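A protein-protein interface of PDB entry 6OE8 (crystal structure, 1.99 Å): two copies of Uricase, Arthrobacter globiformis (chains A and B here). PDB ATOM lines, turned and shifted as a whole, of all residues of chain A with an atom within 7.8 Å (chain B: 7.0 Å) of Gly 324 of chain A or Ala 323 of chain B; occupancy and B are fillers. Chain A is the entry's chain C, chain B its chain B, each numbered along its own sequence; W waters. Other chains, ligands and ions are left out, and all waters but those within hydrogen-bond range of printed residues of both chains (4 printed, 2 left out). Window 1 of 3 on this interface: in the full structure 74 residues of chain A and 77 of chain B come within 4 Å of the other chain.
NH2 of Arg 131 of chain B lies within hydrogen-bond range of O of Ile 322 of chain B, at 3.2 Å.
The side-chain carboxylate of Glu 304 of chain B lies within hydrogen-bond range of the side-chain hydroxyl of Ser 270 of chain B (2.4 Å).
O of Gln 71 of chain A is in hydrogen-bond range of N of Arg 131 of chain A (2.9 Å).
NH2 of Arg 131 of chain A is in hydrogen-bond range of O of Ile 322 of chain A (3.2 Å).
Among the printed residues, pairs that only touch across the chains: Trp 319 of chain A with Ser 320 of chain B, Ser 320 of chain A with Ser 320 of chain B, Ile 322 of chain A with Cys 326 of chain B, Ala 323 of chain A with Ala 323 of chain B, Ala 323 of chain A with Gly 324 of chain B, Gly 324 of chain A with Ala 323 of chain B, Phe 325 of chain A with Glu 304 of chain B, Cys 326 of chain A with Ile 322 of chain B and Cys 326 of chain A with Ala 323 of chain B.
Gly 324 of chain A touches one residue of chain B.
Ala 323 of chain B touches three residues of chain A.
Printed residues of chain A within 4 Å of Ile 322 of chain B: Cys 326 (3.8 Å).
Of the printed residues of chain A, Glu 304 of chain B touches Gln 43 (2.9 Å), Gln 71 (3.0 Å) and Phe 325 (3.2 Å).
The nearest residue of chain B that does not touch Gly 324 of chain A is Glu 304 of chain B (5.4 Å).
The nearest residue of chain A that does not touch Ala 323 of chain B is Phe 325 of chain A (4.8 Å).
Hydrophobic or aromatic side chains of chain B that line the printed part of chain A: Ile 322 and Ala 323.
Among the printed residues, 14 pairs touch across the chains.
Trp 319 of chain A touches Ser 320 of chain B, but with the chains exchanged Ser 320 of chain A does not touch Trp 319 of chain B (4.1 Å).
Ser 320 of chain B touches its own counterpart, Ser 320 of chain A.
Ile 322 of chain A touches Cys 326 of chain B, and with the chains exchanged Cys 326 of chain A touches Ile 322 of chain B.
Ala 323 of chain A touches its own counterpart, Ala 323 of chain B.
Of the 14 pairs that touch across the chains among the printed residues, 8 have their exchanged pair printed and touching as well.
The guanidinium group of Arg 213 of chain B lies within salt-bridge range of the chain-end carboxylate of Cys 326 of chain A (2.7 Å).
The backbone NH (N) of Ser 270 of chain B lies within hydrogen-bond range of the side-chain sulfur (SG) of Cys 326 of chain A (3.6 Å).
The backbone NH (N) of Glu 304 of chain B sits at hydrogen-bond distance from the backbone carbonyl oxygen (O) of Gln 43 of chain A (2.9 Å).
The side-chain carboxylate (OE1) of Glu 304 of chain B lies within hydrogen-bond range of the side-chain amide nitrogen (NE2) of Gln 71 of chain A, at 3.0 Å.
The guanidinium group (NE) of Arg 213 of chain A lies within salt-bridge range of the chain-end carboxylate (O) of Cys 326 of chain B.
Water W1 lies within hydrogen-bond range of OE2 of Glu 304 of chain B (2.5 Å) and N of Phe 325 of chain A (2.7 Å).
Water W2 bridges the chain-end carboxylate of Cys 326 of chain B and the guanidinium group of Arg 213 of chain A.
Water W3 lies within hydrogen-bond range of OE1 of Glu 304 of chain B (2.7 Å), OE1 of Gln 71 of chain A (2.7 Å) and NE2 of Gln 43 of chain A (3.4 Å).
Water W4 lies within hydrogen-bond range of the backbone carbonyl oxygen of Glu 304 of chain B (2.9 Å) and the backbone carbonyl oxygen of Gln 43 of chain A (3.4 Å).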
ATOM      1  N   GLN A  43      24.952   1.848   3.255  1.00  0.00           N
ATOM      2  CA  GLN A  43      23.755   2.434   3.840  1.00  0.00           C
ATOM      3  C   GLN A  43      22.625   1.446   3.619  1.00  0.00           C
ATOM      4  O   GLN A  43      22.677   0.646   2.684  1.00  0.00           O
ATOM      5  CB  GLN A  43      23.438   3.795   3.202  1.00  0.00           C
ATOM      6  CG  GLN A  43      23.097   3.730   1.713  1.00  0.00           C
ATOM      7  CD  GLN A  43      23.100   5.091   1.028  1.00  0.00           C
ATOM      8  OE1 GLN A  43      23.458   6.108   1.632  1.00  0.00           O
ATOM      9  NE2 GLN A  43      22.654   5.126  -0.226  1.00  0.00           N
ATOM     10  N   GLN A  71      17.128   5.453   4.922  1.00  0.00           N
ATOM     11  CA  GLN A  71      18.355   4.669   4.940  1.00  0.00           C
ATOM     12  C   GLN A  71      19.291   5.199   6.022  1.00  0.00           C
ATOM     13  O   GLN A  71      19.407   6.411   6.208  1.00  0.00           O
ATOM     14  CB  GLN A  71      19.013   4.696   3.576  1.00  0.00           C
ATOM     15  CG  GLN A  71      18.305   3.788   2.561  1.00  0.00           C
ATOM     16  CD  GLN A  71      19.021   3.752   1.242  1.00  0.00           C
ATOM     17  OE1 GLN A  71      19.276   4.796   0.636  1.00  0.00           O
ATOM     18  NE2 GLN A  71      19.418   2.559   0.820  1.00  0.00           N
ATOM     19  N   ARG A 131      20.289   8.930   5.069  1.00  0.00           N
ATOM     20  CA  ARG A 131      19.685   9.576   3.909  1.00  0.00           C
ATOM     21  C   ARG A 131      18.198   9.254   3.907  1.00  0.00           C
ATOM     22  O   ARG A 131      17.813   8.082   3.848  1.00  0.00           O
ATOM     23  CB  ARG A 131      20.340   9.092   2.612  1.00  0.00           C
ATOM     24  CG  ARG A 131      19.803   9.747   1.343  1.00  0.00           C
ATOM     25  CD  ARG A 131      20.420   9.122   0.103  1.00  0.00           C
ATOM     26  NE  ARG A 131      19.967   9.756  -1.137  1.00  0.00           N
ATOM     27  CZ  ARG A 131      18.848   9.434  -1.784  1.00  0.00           C
ATOM     28  NH1 ARG A 131      18.042   8.507  -1.290  1.00  0.00           N
ATOM     29  NH2 ARG A 131      18.520  10.055  -2.911  1.00  0.00           N
ATOM     30  N   ARG A 213      17.136  20.334  -8.738  1.00  0.00           N
ATOM     31  CA  ARG A 213      17.332  20.076  -7.316  1.00  0.00           C
ATOM     32  C   ARG A 213      18.208  21.189  -6.762  1.00  0.00           C
ATOM     33  O   ARG A 213      19.234  21.514  -7.360  1.00  0.00           O
ATOM     34  CB  ARG A 213      17.983  18.699  -7.078  1.00  0.00           C
ATOM     35  CG  ARG A 213      17.092  17.462  -7.390  1.00  0.00           C
ATOM     36  CD  ARG A 213      17.843  16.147  -7.080  1.00  0.00           C
ATOM     37  NE  ARG A 213      17.157  14.920  -7.501  1.00  0.00           N
ATOM     38  CZ  ARG A 213      16.377  14.156  -6.739  1.00  0.00           C
ATOM     39  NH1 ARG A 213      16.171  14.449  -5.467  1.00  0.00           N
ATOM     40  NH2 ARG A 213      15.822  13.066  -7.259  1.00  0.00           N
ATOM     41  N   ILE A 318      26.262  15.341  -0.361  1.00  0.00           N
ATOM     42  CA  ILE A 318      24.914  14.836  -0.617  1.00  0.00           C
ATOM     43  C   ILE A 318      24.722  14.523  -2.103  1.00  0.00           C
ATOM     44  O   ILE A 318      24.105  13.502  -2.462  1.00  0.00           O
ATOM     45  CB  ILE A 318      23.876  15.859  -0.095  1.00  0.00           C
ATOM     46  CG1 ILE A 318      22.456  15.259  -0.049  1.00  0.00           C
ATOM     47  CG2 ILE A 318      23.929  17.173  -0.889  1.00  0.00           C
ATOM     48  CD1 ILE A 318      21.457  16.143   0.684  1.00  0.00           C
ATOM     49  N   TRP A 319      25.409  15.269  -2.976  1.00  0.00           N
ATOM     50  CA  TRP A 319      25.236  15.047  -4.405  1.00  0.00           C
ATOM     51  C   TRP A 319      25.796  13.704  -4.838  1.00  0.00           C
ATOM     52  O   TRP A 319      25.387  13.184  -5.887  1.00  0.00           O
ATOM     53  CB  TRP A 319      25.896  16.164  -5.218  1.00  0.00           C
ATOM     54  CG  TRP A 319      25.323  17.526  -4.972  1.00  0.00           C
ATOM     55  CD1 TRP A 319      25.930  18.576  -4.351  1.00  0.00           C
ATOM     56  CD2 TRP A 319      23.989  17.950  -5.268  1.00  0.00           C
ATOM     57  NE1 TRP A 319      25.068  19.654  -4.295  1.00  0.00           N
ATOM     58  CE2 TRP A 319      23.869  19.288  -4.849  1.00  0.00           C
ATOM     59  CE3 TRP A 319      22.891  17.334  -5.874  1.00  0.00           C
ATOM     60  CZ2 TRP A 319      22.692  20.019  -5.013  1.00  0.00           C
ATOM     61  CZ3 TRP A 319      21.727  18.059  -6.033  1.00  0.00           C
ATOM     62  CH2 TRP A 319      21.634  19.383  -5.600  1.00  0.00           C
ATOM     63  N   SER A 320      26.694  13.115  -4.047  1.00  0.00           N
ATOM     64  CA  SER A 320      27.268  11.840  -4.454  1.00  0.00           C
ATOM     65  C   SER A 320      26.211  10.748  -4.513  1.00  0.00           C
ATOM     66  O   SER A 320      26.337   9.818  -5.314  1.00  0.00           O
ATOM     67  CB  SER A 320      28.392  11.430  -3.508  1.00  0.00           C
ATOM     68  OG  SER A 320      29.458  12.372  -3.558  1.00  0.00           O
ATOM     69  N   ASN A 321      25.170  10.821  -3.684  1.00  0.00           N
ATOM     70  CA  ASN A 321      24.163   9.764  -3.729  1.00  0.00           C
ATOM     71  C   ASN A 321      22.780  10.280  -4.107  1.00  0.00           C
ATOM     72  O   ASN A 321      21.786   9.567  -3.927  1.00  0.00           O
ATOM     73  CB  ASN A 321      24.132   8.982  -2.414  1.00  0.00           C
ATOM     74  CG  ASN A 321      25.470   8.342  -2.101  1.00  0.00           C
ATOM     75  OD1 ASN A 321      26.080   8.614  -1.067  1.00  0.00           O
ATOM     76  ND2 ASN A 321      25.935   7.479  -3.004  1.00  0.00           N
ATOM     77  N   ILE A 322      22.701  11.474  -4.694  1.00  0.00           N
ATOM     78  CA  ILE A 322      21.401  12.097  -4.881  1.00  0.00           C
ATOM     79  C   ILE A 322      20.566  11.328  -5.909  1.00  0.00           C
ATOM     80  O   ILE A 322      19.336  11.263  -5.793  1.00  0.00           O
ATOM     81  CB  ILE A 322      21.606  13.573  -5.268  1.00  0.00           C
ATOM     82  CG1 ILE A 322      20.321  14.370  -5.056  1.00  0.00           C
ATOM     83  CG2 ILE A 322      22.110  13.695  -6.713  1.00  0.00           C
ATOM     84  CD1 ILE A 322      19.974  14.534  -3.590  1.00  0.00           C
ATOM     85  N   ALA A 323      21.206  10.725  -6.910  1.00  0.00           N
ATOM     86  CA  ALA A 323      20.510   9.975  -7.946  1.00  0.00           C
ATOM     87  C   ALA A 323      20.528   8.477  -7.687  1.00  0.00           C
ATOM     88  O   ALA A 323      19.941   7.719  -8.465  1.00  0.00           O
ATOM     89  CB  ALA A 323      21.124  10.272  -9.320  1.00  0.00           C
ATOM     90  N   GLY A 324      21.173   8.039  -6.610  1.00  0.00           N
ATOM     91  CA  GLY A 324      21.300   6.629  -6.303  1.00  0.00           C
ATOM     92  C   GLY A 324      22.696   6.260  -5.845  1.00  0.00           C
ATOM     93  O   GLY A 324      23.637   7.047  -5.996  1.00  0.00           O
ATOM     94  N   PHE A 325      22.840   5.059  -5.285  1.00  0.00           N
ATOM     95  CA  PHE A 325      24.112   4.618  -4.720  1.00  0.00           C
ATOM     96  C   PHE A 325      25.067   4.146  -5.809  1.00  0.00           C
ATOM     97  O   PHE A 325      26.257   4.480  -5.783  1.00  0.00           O
ATOM     98  CB  PHE A 325      23.851   3.489  -3.719  1.00  0.00           C
ATOM     99  CG  PHE A 325      25.079   2.978  -3.021  1.00  0.00           C
ATOM    100  CD1 PHE A 325      25.637   3.680  -1.956  1.00  0.00           C
ATOM    101  CD2 PHE A 325      25.671   1.787  -3.429  1.00  0.00           C
ATOM    102  CE1 PHE A 325      26.755   3.203  -1.306  1.00  0.00           C
ATOM    103  CE2 PHE A 325      26.794   1.305  -2.792  1.00  0.00           C
ATOM    104  CZ  PHE A 325      27.342   2.019  -1.721  1.00  0.00           C
ATOM    105  N   CYS A 326      24.565   3.357  -6.755  1.00  0.00           N
ATOM    106  CA  CYS A 326      25.363   2.854  -7.868  1.00  0.00           C
ATOM    107  C   CYS A 326      24.435   2.418  -9.000  1.00  0.00           C
ATOM    108  O   CYS A 326      23.292   2.876  -9.087  1.00  0.00           O
ATOM    109  CB  CYS A 326      26.244   1.685  -7.421  1.00  0.00           C
ATOM    110  SG  CYS A 326      25.323   0.198  -6.900  1.00  0.00           S
ATOM    111  OXT CYS A 326      24.784   1.581  -9.831  1.00  0.00           O
ATOM    112  N   ARG B 131      32.184  11.778 -19.832  1.00  0.00           N
ATOM    113  CA  ARG B 131      31.564  10.555 -19.338  1.00  0.00           C
ATOM    114  C   ARG B 131      30.867   9.881 -20.510  1.00  0.00           C
ATOM    115  O   ARG B 131      29.962  10.465 -21.116  1.00  0.00           O
ATOM    116  CB  ARG B 131      30.552  10.856 -18.226  1.00  0.00           C
ATOM    117  CG  ARG B 131      29.899   9.617 -17.609  1.00  0.00           C
ATOM    118  CD  ARG B 131      28.851  10.001 -16.576  1.00  0.00           C
ATOM    119  NE  ARG B 131      28.231   8.843 -15.924  1.00  0.00           N
ATOM    120  CZ  ARG B 131      27.181   8.176 -16.406  1.00  0.00           C
ATOM    121  NH1 ARG B 131      26.631   8.528 -17.565  1.00  0.00           N
ATOM    122  NH2 ARG B 131      26.683   7.147 -15.733  1.00  0.00           N
ATOM    123  N   ARG B 213      28.434  -2.780  -9.721  1.00  0.00           N
ATOM    124  CA  ARG B 213      29.343  -2.008 -10.558  1.00  0.00           C
ATOM    125  C   ARG B 213      30.729  -2.070  -9.938  1.00  0.00           C
ATOM    126  O   ARG B 213      30.886  -1.796  -8.750  1.00  0.00           O
ATOM    127  CB  ARG B 213      28.887  -0.547 -10.688  1.00  0.00           C
ATOM    128  CG  ARG B 213      27.606  -0.314 -11.508  1.00  0.00           C
ATOM    129  CD  ARG B 213      27.318   1.187 -11.606  1.00  0.00           C
ATOM    130  NE  ARG B 213      26.019   1.514 -12.200  1.00  0.00           N
ATOM    131  CZ  ARG B 213      25.797   1.755 -13.490  1.00  0.00           C
ATOM    132  NH1 ARG B 213      26.787   1.714 -14.369  1.00  0.00           N
ATOM    133  NH2 ARG B 213      24.570   2.046 -13.899  1.00  0.00           N
ATOM    134  N   SER B 270      23.868  -2.546  -5.003  1.00  0.00           N
ATOM    135  CA  SER B 270      22.598  -2.050  -4.488  1.00  0.00           C
ATOM    136  C   SER B 270      21.573  -3.163  -4.637  1.00  0.00           C
ATOM    137  O   SER B 270      21.196  -3.511  -5.760  1.00  0.00           O
ATOM    138  CB  SER B 270      22.157  -0.789  -5.232  1.00  0.00           C
ATOM    139  OG  SER B 270      20.903  -0.346  -4.765  1.00  0.00           O
ATOM    140  N   GLU B 304      22.720  -1.375   0.556  1.00  0.00           N
ATOM    141  CA  GLU B 304      23.741  -0.904  -0.374  1.00  0.00           C
ATOM    142  C   GLU B 304      25.117  -0.894   0.278  1.00  0.00           C
ATOM    143  O   GLU B 304      25.266  -0.464   1.427  1.00  0.00           O
ATOM    144  CB  GLU B 304      23.348   0.487  -0.917  1.00  0.00           C
ATOM    145  CG  GLU B 304      21.899   0.464  -1.469  1.00  0.00           C
ATOM    146  CD  GLU B 304      21.473   1.730  -2.190  1.00  0.00           C
ATOM    147  OE1 GLU B 304      21.341   2.776  -1.517  1.00  0.00           O
ATOM    148  OE2 GLU B 304      21.215   1.657  -3.418  1.00  0.00           O
ATOM    149  N   ILE B 318      34.555   9.012 -10.081  1.00  0.00           N
ATOM    150  CA  ILE B 318      33.623   8.424 -11.047  1.00  0.00           C
ATOM    151  C   ILE B 318      32.308   8.031 -10.392  1.00  0.00           C
ATOM    152  O   ILE B 318      31.252   8.074 -11.033  1.00  0.00           O
ATOM    153  CB  ILE B 318      34.277   7.224 -11.763  1.00  0.00           C
ATOM    154  CG1 ILE B 318      33.463   6.825 -13.003  1.00  0.00           C
ATOM    155  CG2 ILE B 318      34.440   6.045 -10.813  1.00  0.00           C
ATOM    156  CD1 ILE B 318      34.201   5.890 -13.935  1.00  0.00           C
ATOM    157  N   TRP B 319      32.333   7.670  -9.107  1.00  0.00           N
ATOM    158  CA  TRP B 319      31.108   7.236  -8.448  1.00  0.00           C
ATOM    159  C   TRP B 319      30.127   8.376  -8.213  1.00  0.00           C
ATOM    160  O   TRP B 319      28.940   8.115  -7.986  1.00  0.00           O
ATOM    161  CB  TRP B 319      31.420   6.558  -7.109  1.00  0.00           C
ATOM    162  CG  TRP B 319      32.259   5.325  -7.238  1.00  0.00           C
ATOM    163  CD1 TRP B 319      33.561   5.170  -6.853  1.00  0.00           C
ATOM    164  CD2 TRP B 319      31.868   4.085  -7.837  1.00  0.00           C
ATOM    165  NE1 TRP B 319      33.992   3.897  -7.142  1.00  0.00           N
ATOM    166  CE2 TRP B 319      32.974   3.213  -7.755  1.00  0.00           C
ATOM    167  CE3 TRP B 319      30.687   3.623  -8.424  1.00  0.00           C
ATOM    168  CZ2 TRP B 319      32.932   1.907  -8.236  1.00  0.00           C
ATOM    169  CZ3 TRP B 319      30.648   2.327  -8.901  1.00  0.00           C
ATOM    170  CH2 TRP B 319      31.763   1.483  -8.803  1.00  0.00           C
ATOM    171  N   SER B 320      30.590   9.629  -8.247  1.00  0.00           N
ATOM    172  CA  SER B 320      29.702  10.735  -7.903  1.00  0.00           C
ATOM    173  C   SER B 320      28.575  10.903  -8.914  1.00  0.00           C
ATOM    174  O   SER B 320      27.482  11.352  -8.551  1.00  0.00           O
ATOM    175  CB  SER B 320      30.502  12.031  -7.773  1.00  0.00           C
ATOM    176  OG  SER B 320      31.430  11.932  -6.704  1.00  0.00           O
ATOM    177  N   ASN B 321      28.804  10.541 -10.174  1.00  0.00           N
ATOM    178  CA  ASN B 321      27.778  10.671 -11.201  1.00  0.00           C
ATOM    179  C   ASN B 321      27.453   9.330 -11.858  1.00  0.00           C
ATOM    180  O   ASN B 321      26.869   9.298 -12.951  1.00  0.00           O
ATOM    181  CB  ASN B 321      28.200  11.710 -12.239  1.00  0.00           C
ATOM    182  CG  ASN B 321      28.366  13.102 -11.631  1.00  0.00           C
ATOM    183  OD1 ASN B 321      27.469  13.629 -11.010  1.00  0.00           O
ATOM    184  ND2 ASN B 321      29.516  13.694 -11.824  1.00  0.00           N
ATOM    185  N   ILE B 322      27.807   8.219 -11.201  1.00  0.00           N
ATOM    186  CA  ILE B 322      27.629   6.902 -11.809  1.00  0.00           C
ATOM    187  C   ILE B 322      26.150   6.601 -12.027  1.00  0.00           C
ATOM    188  O   ILE B 322      25.786   5.902 -12.982  1.00  0.00           O
ATOM    189  CB  ILE B 322      28.305   5.817 -10.943  1.00  0.00           C
ATOM    190  CG1 ILE B 322      28.555   4.548 -11.752  1.00  0.00           C
ATOM    191  CG2 ILE B 322      27.457   5.471  -9.721  1.00  0.00           C
ATOM    192  CD1 ILE B 322      29.618   4.704 -12.816  1.00  0.00           C
ATOM    193  N   ALA B 323      25.278   7.113 -11.160  1.00  0.00           N
ATOM    194  CA  ALA B 323      23.847   6.858 -11.257  1.00  0.00           C
ATOM    195  C   ALA B 323      23.088   8.003 -11.910  1.00  0.00           C
ATOM    196  O   ALA B 323      21.865   7.909 -12.071  1.00  0.00           O
ATOM    197  CB  ALA B 323      23.265   6.573  -9.866  1.00  0.00           C
ATOM    198  N   GLY B 324      23.779   9.073 -12.290  1.00  0.00           N
ATOM    199  CA  GLY B 324      23.134  10.242 -12.851  1.00  0.00           C
ATOM    200  C   GLY B 324      23.686  11.526 -12.269  1.00  0.00           C
ATOM    201  O   GLY B 324      24.345  11.503 -11.225  1.00  0.00           O
ATOM    202  N   PHE B 325      23.384  12.655 -12.918  1.00  0.00           N
ATOM    203  CA  PHE B 325      23.906  13.954 -12.501  1.00  0.00           C
ATOM    204  C   PHE B 325      23.145  14.500 -11.299  1.00  0.00           C
ATOM    205  O   PHE B 325      23.755  15.002 -10.352  1.00  0.00           O
ATOM    206  CB  PHE B 325      23.822  14.929 -13.676  1.00  0.00           C
ATOM    207  CG  PHE B 325      24.394  16.292 -13.403  1.00  0.00           C
ATOM    208  CD1 PHE B 325      25.767  16.501 -13.402  1.00  0.00           C
ATOM    209  CD2 PHE B 325      23.551  17.370 -13.183  1.00  0.00           C
ATOM    210  CE1 PHE B 325      26.284  17.771 -13.171  1.00  0.00           C
ATOM    211  CE2 PHE B 325      24.054  18.635 -12.949  1.00  0.00           C
ATOM    212  CZ  PHE B 325      25.423  18.840 -12.944  1.00  0.00           C
ATOM    213  N   CYS B 326      21.819  14.418 -11.329  1.00  0.00           N
ATOM    214  CA  CYS B 326      20.991  14.855 -10.215  1.00  0.00           C
ATOM    215  C   CYS B 326      19.643  14.161 -10.318  1.00  0.00           C
ATOM    216  O   CYS B 326      18.870  14.096  -9.367  1.00  0.00           O
ATOM    217  CB  CYS B 326      20.832  16.382 -10.188  1.00  0.00           C
ATOM    218  SG  CYS B 326      19.939  17.116 -11.583  1.00  0.00           S
ATOM    219  OXT CYS B 326      19.289  13.654 -11.379  1.00  0.00           O
HETATM  220  O   HOH W   1      20.618   3.676  -4.740  1.00  0.00           O
HETATM  221  O   HOH W   2      17.121  12.326 -10.125  1.00  0.00           O
HETATM  222  O   HOH W   3      19.782   4.920  -2.017  1.00  0.00           O
HETATM  223  O   HOH W   4      24.393  -2.182   3.573  1.00  0.00           O
